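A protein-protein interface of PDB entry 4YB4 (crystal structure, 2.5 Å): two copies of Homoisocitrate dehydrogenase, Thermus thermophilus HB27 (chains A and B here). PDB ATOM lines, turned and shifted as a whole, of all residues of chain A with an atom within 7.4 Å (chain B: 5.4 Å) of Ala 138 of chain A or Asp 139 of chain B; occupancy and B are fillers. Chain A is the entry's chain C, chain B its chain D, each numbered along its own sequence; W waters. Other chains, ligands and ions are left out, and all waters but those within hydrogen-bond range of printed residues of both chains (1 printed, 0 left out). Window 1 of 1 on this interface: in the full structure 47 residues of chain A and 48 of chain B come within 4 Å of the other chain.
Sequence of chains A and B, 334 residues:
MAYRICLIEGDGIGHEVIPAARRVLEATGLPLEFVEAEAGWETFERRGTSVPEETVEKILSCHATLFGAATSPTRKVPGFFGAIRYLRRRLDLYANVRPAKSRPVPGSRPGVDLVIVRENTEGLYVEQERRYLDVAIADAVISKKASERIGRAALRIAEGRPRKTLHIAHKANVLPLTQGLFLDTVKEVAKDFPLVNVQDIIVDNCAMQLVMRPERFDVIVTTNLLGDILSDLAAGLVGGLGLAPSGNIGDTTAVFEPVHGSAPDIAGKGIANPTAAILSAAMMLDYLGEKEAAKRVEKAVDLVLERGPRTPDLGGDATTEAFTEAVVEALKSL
Water W1 lies within hydrogen-bond range of OD1 of Asp 139 of chain A (2.4 Å), OD1 of Asp 139 of chain B (2.6 Å), NH2 of Arg 130 of chain A (3.2 Å) and NH2 of Arg 130 of chain B (3.4 Å).
CD2 of Leu 124 of chain B touches CD2 of Leu 124 of chain A, at 3.8 Å.
Ala 140 of chain B touches Ala 136 of chain A (O to O, 3.8 Å).
Ala 136 of chain A touches Val 141 of chain B (O to CA, 3.3 Å).
Ala 136 of chain A touches Thr 178 of chain B.
Thr 178 of chain B touches Ala 138 of chain A (CG2 to N, 3.7 Å).
CG2 of Ile 137 of chain B touches OD1 of Asp 139 of chain A, 3.8 Å away.
CD1 of Ile 137 of chain B touches CG2 of Val 141 of chain A, 3.6 Å away.
Leu 175 of chain A touches Leu 124 of chain B.
Glu 129 of chain B touches Leu 175 of chain A.
Thr 178 of chain A touches Ile 137 of chain B (CG2 to C, 3.7 Å).
Gly 123 of chain A touches none of the printed residues of chain B.
Printed residues of chain B within 4 Å of Leu 124 of chain A: Leu 124 and Leu 175.
Gln 128 of chain A touches none of the printed residues of chain B.
Of the printed residues of chain B, Glu 129 of chain A touches Leu 175 and Thr 178.
Printed residues of chain B within 4 Å of Ala 138 of chain A: Ala 138 (3.6 Å), Asp 139 (3.8 Å), Ala 140 (2.9 Å) and Thr 178 (3.7 Å).
Of chain A, only Ile 137 (3.8 Å) and Ala 138 (3.8 Å) come within 4 Å of Asp 139 of chain B.
Of the printed residues of chain A, Thr 178 of chain B touches Glu 129, Ala 136, Ile 137 and Ala 138.
Of the 15 printed residues of chain A, 10 touch a printed residue of chain B.
Hydrophobic or aromatic side chains of chain A that line the printed part of chain B: Leu 124, Ala 136, Ile 137, Ala 138, Ala 140, Val 141 and Leu 175.
Along chain A the printed residues that touch a printed residue of chain B span positions 124 to 178.
Of the 14 printed residues of chain B, 9 touch a printed residue of chain A.
Hydrophobic or aromatic side chains of chain B that line the printed part of chain A: Leu 124, Ile 137, Ala 138, Ala 140, Val 141 and Leu 175.
Among the printed residues, 24 pairs touch across the chains.
Among the printed residues, no Asp or Glu carboxylate lies within 4 Å of a Lys or Arg side-chain nitrogen of the other chain.
Leu 124 of chain A touches Leu 175 of chain B, and with the chains exchanged Leu 175 of chain A touches Leu 124 of chain B.
Glu 129 of chain A touches Leu 175 of chain B, and with the chains exchanged Leu 175 of chain A touches Glu 129 of chain B.
Ile 137 of chain A touches Ala 140 of chain B, and with the chains exchanged Ala 140 of chain A touches Ile 137 of chain B.
Ala 138 of chain A touches Thr 178 of chain B, and with the chains exchanged Thr 178 of chain A touches Ala 138 of chain B.
Positions printed for both chains: 123, 124, 126, 127, 128, 129, 130, 137, 138, 139, 140, 141, 175 and 178.
Of the 24 pairs that touch across the chains among the printed residues, 20 have their exchanged pair printed and touching as well.
N of Arg 130 of chain B sits at hydrogen-bond distance from O of Ile 137 of chain B, at 2.9 Å.
The backbone carbonyl oxygen of Gln 128 of chain A sits at hydrogen-bond distance from the backbone NH of Asp 139 of chain A (3.2 Å).
The backbone carbonyl oxygen (O) of Ile 137 of chain A is in hydrogen-bond range of the backbone NH (N) of Arg 130 of chain A.
The backbone NH of Gly 123 of chain B sits at hydrogen-bond distance from the backbone carbonyl oxygen of Val 141 of chain B (2.8 Å).
O of Gln 128 of chain B sits at hydrogen-bond distance from N of Asp 139 of chain B.
The guanidinium group (NH2) of Arg 130 of chain B lies within salt-bridge range of the side-chain carboxylate (OD1) of Asp 139 of chain B (2.6 Å).
OE1 of Glu 129 of chain A lies within hydrogen-bond range of OG1 of Thr 178 of chain B (2.5 Å).
The side-chain carboxylate (OE1) of Glu 129 of chain B sits at hydrogen-bond distance from the side-chain hydroxyl (OG1) of Thr 178 of chain A, 2.6 Å away.
O of Ala 140 of chain B is in hydrogen-bond range of N of Ala 138 of chain A, at 2.9 Å.
The backbone NH (N) of Ala 138 of chain B is in hydrogen-bond range of the backbone carbonyl oxygen (O) of Ala 140 of chain A (2.9 Å).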
ATOM      1  N   GLY A 123       9.793  27.091  15.780  1.00  0.00           N
ATOM      2  CA  GLY A 123       9.886  27.097  14.337  1.00  0.00           C
ATOM      3  C   GLY A 123      10.917  28.110  13.871  1.00  0.00           C
ATOM      4  O   GLY A 123      11.959  28.264  14.476  1.00  0.00           O
ATOM      5  N   LEU A 124      10.578  28.841  12.827  1.00  0.00           N
ATOM      6  CA  LEU A 124      11.406  29.897  12.290  1.00  0.00           C
ATOM      7  C   LEU A 124      11.476  31.096  13.243  1.00  0.00           C
ATOM      8  O   LEU A 124      12.384  31.916  13.111  1.00  0.00           O
ATOM      9  CB  LEU A 124      10.845  30.381  10.951  1.00  0.00           C
ATOM     10  CG  LEU A 124      11.388  30.028   9.558  1.00  0.00           C
ATOM     11  CD1 LEU A 124      12.823  29.520   9.574  1.00  0.00           C
ATOM     12  CD2 LEU A 124      10.479  29.096   8.789  1.00  0.00           C
ATOM     13  N   VAL A 126      12.351  31.426  16.161  1.00  0.00           N
ATOM     14  CA  VAL A 126      13.392  31.253  17.133  1.00  0.00           C
ATOM     15  C   VAL A 126      14.383  32.400  16.939  1.00  0.00           C
ATOM     16  O   VAL A 126      15.122  32.738  17.838  1.00  0.00           O
ATOM     17  CB  VAL A 126      13.988  29.855  16.891  1.00  0.00           C
ATOM     18  CG1 VAL A 126      15.357  29.917  16.285  1.00  0.00           C
ATOM     19  CG2 VAL A 126      13.902  28.995  18.126  1.00  0.00           C
ATOM     20  N   GLU A 127      14.366  33.018  15.760  1.00  0.00           N
ATOM     21  CA  GLU A 127      15.252  34.127  15.442  1.00  0.00           C
ATOM     22  C   GLU A 127      16.706  33.894  15.804  1.00  0.00           C
ATOM     23  O   GLU A 127      17.264  34.528  16.686  1.00  0.00           O
ATOM     24  CB  GLU A 127      14.742  35.456  16.014  1.00  0.00           C
ATOM     25  CG  GLU A 127      14.372  36.454  14.906  1.00  0.00           C
ATOM     26  CD  GLU A 127      14.595  37.894  15.333  1.00  0.00           C
ATOM     27  OE1 GLU A 127      14.142  38.225  16.466  1.00  0.00           O
ATOM     28  OE2 GLU A 127      15.224  38.674  14.550  1.00  0.00           O
ATOM     29  N   GLN A 128      17.297  32.944  15.096  1.00  0.00           N
ATOM     30  CA  GLN A 128      18.708  32.684  15.165  1.00  0.00           C
ATOM     31  C   GLN A 128      19.222  32.723  13.740  1.00  0.00           C
ATOM     32  O   GLN A 128      19.463  31.686  13.124  1.00  0.00           O
ATOM     33  CB  GLN A 128      18.940  31.334  15.837  1.00  0.00           C
ATOM     34  CG  GLN A 128      18.591  31.360  17.312  1.00  0.00           C
ATOM     35  CD  GLN A 128      19.472  32.318  18.107  1.00  0.00           C
ATOM     36  OE1 GLN A 128      20.558  32.718  17.670  1.00  0.00           O
ATOM     37  NE2 GLN A 128      19.007  32.687  19.275  1.00  0.00           N
ATOM     38  N   GLU A 129      19.329  33.941  13.209  1.00  0.00           N
ATOM     39  CA  GLU A 129      19.864  34.156  11.872  1.00  0.00           C
ATOM     40  C   GLU A 129      21.330  34.569  11.889  1.00  0.00           C
ATOM     41  O   GLU A 129      21.795  35.194  12.836  1.00  0.00           O
ATOM     42  CB  GLU A 129      19.090  35.259  11.147  1.00  0.00           C
ATOM     43  CG  GLU A 129      17.614  35.005  10.981  1.00  0.00           C
ATOM     44  CD  GLU A 129      16.975  36.003  10.040  1.00  0.00           C
ATOM     45  OE1 GLU A 129      16.703  35.609   8.887  1.00  0.00           O
ATOM     46  OE2 GLU A 129      16.769  37.174  10.449  1.00  0.00           O
ATOM     47  N   ARG A 130      22.011  34.270  10.790  1.00  0.00           N
ATOM     48  CA  ARG A 130      23.425  34.550  10.610  1.00  0.00           C
ATOM     49  C   ARG A 130      23.679  34.893   9.162  1.00  0.00           C
ATOM     50  O   ARG A 130      23.017  34.378   8.269  1.00  0.00           O
ATOM     51  CB  ARG A 130      24.241  33.291  10.918  1.00  0.00           C
ATOM     52  CG  ARG A 130      24.132  32.792  12.343  1.00  0.00           C
ATOM     53  CD  ARG A 130      24.162  31.277  12.380  1.00  0.00           C
ATOM     54  NE  ARG A 130      22.832  30.744  12.259  1.00  0.00           N
ATOM     55  CZ  ARG A 130      22.513  29.500  11.927  1.00  0.00           C
ATOM     56  NH1 ARG A 130      23.423  28.561  11.689  1.00  0.00           N
ATOM     57  NH2 ARG A 130      21.227  29.213  11.864  1.00  0.00           N
ATOM     58  N   ALA A 136      22.836  33.813   3.823  1.00  0.00           N
ATOM     59  CA  ALA A 136      22.188  33.971   5.113  1.00  0.00           C
ATOM     60  C   ALA A 136      21.511  32.675   5.533  1.00  0.00           C
ATOM     61  O   ALA A 136      20.969  31.958   4.698  1.00  0.00           O
ATOM     62  CB  ALA A 136      21.171  35.084   5.028  1.00  0.00           C
ATOM     63  N   ILE A 137      21.502  32.396   6.836  1.00  0.00           N
ATOM     64  CA  ILE A 137      20.979  31.134   7.367  1.00  0.00           C
ATOM     65  C   ILE A 137      20.176  31.413   8.623  1.00  0.00           C
ATOM     66  O   ILE A 137      20.692  32.040   9.561  1.00  0.00           O
ATOM     67  CB  ILE A 137      22.110  30.176   7.790  1.00  0.00           C
ATOM     68  CG1 ILE A 137      23.127  29.985   6.684  1.00  0.00           C
ATOM     69  CG2 ILE A 137      21.567  28.817   8.208  1.00  0.00           C
ATOM     70  CD1 ILE A 137      24.367  29.257   7.178  1.00  0.00           C
ATOM     71  N   ALA A 138      18.939  30.917   8.660  1.00  0.00           N
ATOM     72  CA  ALA A 138      18.120  30.943   9.866  1.00  0.00           C
ATOM     73  C   ALA A 138      17.834  29.520  10.355  1.00  0.00           C
ATOM     74  O   ALA A 138      17.690  28.601   9.548  1.00  0.00           O
ATOM     75  CB  ALA A 138      16.824  31.653   9.574  1.00  0.00           C
ATOM     76  N   ASP A 139      17.752  29.347  11.679  1.00  0.00           N
ATOM     77  CA  ASP A 139      17.329  28.095  12.272  1.00  0.00           C
ATOM     78  C   ASP A 139      15.805  27.982  12.224  1.00  0.00           C
ATOM     79  O   ASP A 139      15.091  28.953  12.496  1.00  0.00           O
ATOM     80  CB  ASP A 139      17.745  28.026  13.731  1.00  0.00           C
ATOM     81  CG  ASP A 139      19.241  27.704  13.937  1.00  0.00           C
ATOM     82  OD1 ASP A 139      19.964  27.309  12.989  1.00  0.00           O
ATOM     83  OD2 ASP A 139      19.664  27.815  15.109  1.00  0.00           O
ATOM     84  N   ALA A 140      15.314  26.801  11.853  1.00  0.00           N
ATOM     85  CA  ALA A 140      13.927  26.423  12.043  1.00  0.00           C
ATOM     86  C   ALA A 140      13.984  25.258  13.021  1.00  0.00           C
ATOM     87  O   ALA A 140      14.503  24.178  12.689  1.00  0.00           O
ATOM     88  CB  ALA A 140      13.305  26.001  10.735  1.00  0.00           C
ATOM     89  N   VAL A 141      13.474  25.478  14.229  1.00  0.00           N
ATOM     90  CA  VAL A 141      13.592  24.518  15.314  1.00  0.00           C
ATOM     91  C   VAL A 141      12.244  23.963  15.741  1.00  0.00           C
ATOM     92  O   VAL A 141      11.305  24.707  15.970  1.00  0.00           O
ATOM     93  CB  VAL A 141      14.271  25.188  16.516  1.00  0.00           C
ATOM     94  CG1 VAL A 141      14.331  24.264  17.729  1.00  0.00           C
ATOM     95  CG2 VAL A 141      15.667  25.608  16.115  1.00  0.00           C
ATOM     96  N   LEU A 175      10.389  18.132   4.948  1.00  0.00           N
ATOM     97  CA  LEU A 175      11.151  18.364   6.176  1.00  0.00           C
ATOM     98  C   LEU A 175      10.787  17.292   7.211  1.00  0.00           C
ATOM     99  O   LEU A 175      10.107  17.569   8.216  1.00  0.00           O
ATOM    100  CB  LEU A 175      10.861  19.767   6.729  1.00  0.00           C
ATOM    101  CG  LEU A 175      11.270  20.958   5.862  1.00  0.00           C
ATOM    102  CD1 LEU A 175      10.808  22.252   6.489  1.00  0.00           C
ATOM    103  CD2 LEU A 175      12.770  21.000   5.666  1.00  0.00           C
ATOM    104  N   THR A 178      12.145  17.928  11.181  1.00  0.00           N
ATOM    105  CA  THR A 178      11.510  18.988  11.975  1.00  0.00           C
ATOM    106  C   THR A 178       9.980  18.961  11.915  1.00  0.00           C
ATOM    107  O   THR A 178       9.307  18.830  12.936  1.00  0.00           O
ATOM    108  CB  THR A 178      11.976  20.362  11.526  1.00  0.00           C
ATOM    109  OG1 THR A 178      11.783  20.495  10.112  1.00  0.00           O
ATOM    110  CG2 THR A 178      13.447  20.547  11.864  1.00  0.00           C
ATOM    111  N   GLY B 123      16.051  28.218   0.365  1.00  0.00           N
ATOM    112  CA  GLY B 123      15.131  28.372   1.464  1.00  0.00           C
ATOM    113  C   GLY B 123      15.202  27.178   2.393  1.00  0.00           C
ATOM    114  O   GLY B 123      16.284  26.684   2.689  1.00  0.00           O
ATOM    115  N   LEU B 124      14.039  26.747   2.876  1.00  0.00           N
ATOM    116  CA  LEU B 124      13.909  25.538   3.663  1.00  0.00           C
ATOM    117  C   LEU B 124      14.174  24.320   2.793  1.00  0.00           C
ATOM    118  O   LEU B 124      14.504  23.243   3.317  1.00  0.00           O
ATOM    119  CB  LEU B 124      12.494  25.403   4.237  1.00  0.00           C
ATOM    120  CG  LEU B 124      12.096  25.769   5.675  1.00  0.00           C
ATOM    121  CD1 LEU B 124      13.292  25.763   6.614  1.00  0.00           C
ATOM    122  CD2 LEU B 124      11.348  27.080   5.747  1.00  0.00           C
ATOM    123  N   VAL B 126      16.485  23.518   0.976  1.00  0.00           N
ATOM    124  CA  VAL B 126      17.889  23.103   1.056  1.00  0.00           C
ATOM    125  C   VAL B 126      18.010  21.764   1.768  1.00  0.00           C
ATOM    126  O   VAL B 126      18.974  21.062   1.610  1.00  0.00           O
ATOM    127  CB  VAL B 126      18.659  24.224   1.806  1.00  0.00           C
ATOM    128  CG1 VAL B 126      19.276  23.772   3.111  1.00  0.00           C
ATOM    129  CG2 VAL B 126      19.638  24.940   0.895  1.00  0.00           C
ATOM    130  N   GLU B 127      17.007  21.443   2.566  1.00  0.00           N
ATOM    131  CA  GLU B 127      16.875  20.180   3.282  1.00  0.00           C
ATOM    132  C   GLU B 127      18.127  19.717   4.004  1.00  0.00           C
ATOM    133  O   GLU B 127      18.726  18.713   3.667  1.00  0.00           O
ATOM    134  CB  GLU B 127      16.285  19.073   2.402  1.00  0.00           C
ATOM    135  CG  GLU B 127      15.390  18.158   3.241  1.00  0.00           C
ATOM    136  CD  GLU B 127      15.138  16.805   2.604  1.00  0.00           C
ATOM    137  OE1 GLU B 127      15.169  16.724   1.341  1.00  0.00           O
ATOM    138  OE2 GLU B 127      14.910  15.834   3.376  1.00  0.00           O
ATOM    139  N   GLN B 128      18.503  20.484   5.013  1.00  0.00           N
ATOM    140  CA  GLN B 128      19.669  20.213   5.812  1.00  0.00           C
ATOM    141  C   GLN B 128      19.179  20.251   7.251  1.00  0.00           C
ATOM    142  O   GLN B 128      19.191  21.295   7.917  1.00  0.00           O
ATOM    143  CB  GLN B 128      20.752  21.256   5.543  1.00  0.00           C
ATOM    144  CG  GLN B 128      21.313  21.189   4.131  1.00  0.00           C
ATOM    145  CD  GLN B 128      22.158  19.950   3.891  1.00  0.00           C
ATOM    146  OE1 GLN B 128      22.790  19.434   4.799  1.00  0.00           O
ATOM    147  NE2 GLN B 128      22.174  19.481   2.665  1.00  0.00           N
ATOM    148  N   GLU B 129      18.718  19.082   7.685  1.00  0.00           N
ATOM    149  CA  GLU B 129      18.068  18.900   8.962  1.00  0.00           C
ATOM    150  C   GLU B 129      18.881  17.976   9.845  1.00  0.00           C
ATOM    151  O   GLU B 129      19.530  17.044   9.368  1.00  0.00           O
ATOM    152  CB  GLU B 129      16.703  18.237   8.773  1.00  0.00           C
ATOM    153  CG  GLU B 129      15.681  18.993   7.962  1.00  0.00           C
ATOM    154  CD  GLU B 129      14.298  18.395   8.175  1.00  0.00           C
ATOM    155  OE1 GLU B 129      13.496  18.995   8.955  1.00  0.00           O
ATOM    156  OE2 GLU B 129      14.054  17.293   7.613  1.00  0.00           O
ATOM    157  N   ARG B 130      18.800  18.203  11.146  1.00  0.00           N
ATOM    158  CA  ARG B 130      19.472  17.364  12.101  1.00  0.00           C
ATOM    159  C   ARG B 130      18.574  17.188  13.276  1.00  0.00           C
ATOM    160  O   ARG B 130      17.751  18.069  13.569  1.00  0.00           O
ATOM    161  CB  ARG B 130      20.734  18.050  12.578  1.00  0.00           C
ATOM    162  CG  ARG B 130      21.666  18.470  11.456  1.00  0.00           C
ATOM    163  CD  ARG B 130      22.168  19.880  11.661  1.00  0.00           C
ATOM    164  NE  ARG B 130      21.449  20.836  10.849  1.00  0.00           N
ATOM    165  CZ  ARG B 130      21.400  22.144  11.072  1.00  0.00           C
ATOM    166  NH1 ARG B 130      22.023  22.711  12.105  1.00  0.00           N
ATOM    167  NH2 ARG B 130      20.710  22.892  10.228  1.00  0.00           N
ATOM    168  N   ILE B 137      16.461  20.634  14.007  1.00  0.00           N
ATOM    169  CA  ILE B 137      16.846  21.913  13.388  1.00  0.00           C
ATOM    170  C   ILE B 137      16.939  21.719  11.889  1.00  0.00           C
ATOM    171  O   ILE B 137      17.472  20.723  11.419  1.00  0.00           O
ATOM    172  CB  ILE B 137      18.269  22.364  13.759  1.00  0.00           C
ATOM    173  CG1 ILE B 137      18.614  21.993  15.185  1.00  0.00           C
ATOM    174  CG2 ILE B 137      18.448  23.859  13.538  1.00  0.00           C
ATOM    175  CD1 ILE B 137      17.762  22.729  16.188  1.00  0.00           C
ATOM    176  N   ALA B 138      16.452  22.698  11.145  1.00  0.00           N
ATOM    177  CA  ALA B 138      16.620  22.744   9.695  1.00  0.00           C
ATOM    178  C   ALA B 138      17.185  24.098   9.292  1.00  0.00           C
ATOM    179  O   ALA B 138      16.793  25.129   9.863  1.00  0.00           O
ATOM    180  CB  ALA B 138      15.291  22.515   9.016  1.00  0.00           C
ATOM    181  N   ASP B 139      18.111  24.102   8.332  1.00  0.00           N
ATOM    182  CA  ASP B 139      18.583  25.356   7.746  1.00  0.00           C
ATOM    183  C   ASP B 139      17.515  25.972   6.827  1.00  0.00           C
ATOM    184  O   ASP B 139      16.935  25.300   5.989  1.00  0.00           O
ATOM    185  CB  ASP B 139      19.834  25.140   6.893  1.00  0.00           C
ATOM    186  CG  ASP B 139      21.120  24.941   7.707  1.00  0.00           C
ATOM    187  OD1 ASP B 139      21.139  25.115   8.962  1.00  0.00           O
ATOM    188  OD2 ASP B 139      22.140  24.620   7.041  1.00  0.00           O
ATOM    189  N   ALA B 140      17.256  27.250   6.996  1.00  0.00           N
ATOM    190  CA  ALA B 140      16.588  28.038   5.985  1.00  0.00           C
ATOM    191  C   ALA B 140      17.634  28.972   5.414  1.00  0.00           C
ATOM    192  O   ALA B 140      18.137  29.845   6.132  1.00  0.00           O
ATOM    193  CB  ALA B 140      15.453  28.846   6.590  1.00  0.00           C
ATOM    194  N   VAL B 141      17.949  28.793   4.135  1.00  0.00           N
ATOM    195  CA  VAL B 141      19.063  29.478   3.512  1.00  0.00           C
ATOM    196  C   VAL B 141      18.632  30.402   2.384  1.00  0.00           C
ATOM    197  O   VAL B 141      17.957  29.967   1.423  1.00  0.00           O
ATOM    198  CB  VAL B 141      20.037  28.452   2.909  1.00  0.00           C
ATOM    199  CG1 VAL B 141      21.163  29.149   2.159  1.00  0.00           C
ATOM    200  CG2 VAL B 141      20.589  27.565   3.998  1.00  0.00           C
ATOM    201  N   LEU B 175      12.308  37.856   9.814  1.00  0.00           N
ATOM    202  CA  LEU B 175      13.603  37.277   9.412  1.00  0.00           C
ATOM    203  C   LEU B 175      14.402  38.245   8.531  1.00  0.00           C
ATOM    204  O   LEU B 175      14.515  38.048   7.308  1.00  0.00           O
ATOM    205  CB  LEU B 175      13.354  35.971   8.661  1.00  0.00           C
ATOM    206  CG  LEU B 175      12.680  34.864   9.474  1.00  0.00           C
ATOM    207  CD1 LEU B 175      11.978  33.838   8.586  1.00  0.00           C
ATOM    208  CD2 LEU B 175      13.686  34.169  10.363  1.00  0.00           C
ATOM    209  N   THR B 178      17.537  36.644   6.454  1.00  0.00           N
ATOM    210  CA  THR B 178      17.244  35.747   5.327  1.00  0.00           C
ATOM    211  C   THR B 178      16.203  36.353   4.395  1.00  0.00           C
ATOM    212  O   THR B 178      16.495  36.653   3.226  1.00  0.00           O
ATOM    213  CB  THR B 178      16.790  34.363   5.794  1.00  0.00           C
ATOM    214  OG1 THR B 178      15.800  34.511   6.811  1.00  0.00           O
ATOM    215  CG2 THR B 178      17.970  33.584   6.334  1.00  0.00           C
HETATM  216  O   HOH W   1      21.284  26.024  11.394  1.00  0.00           O
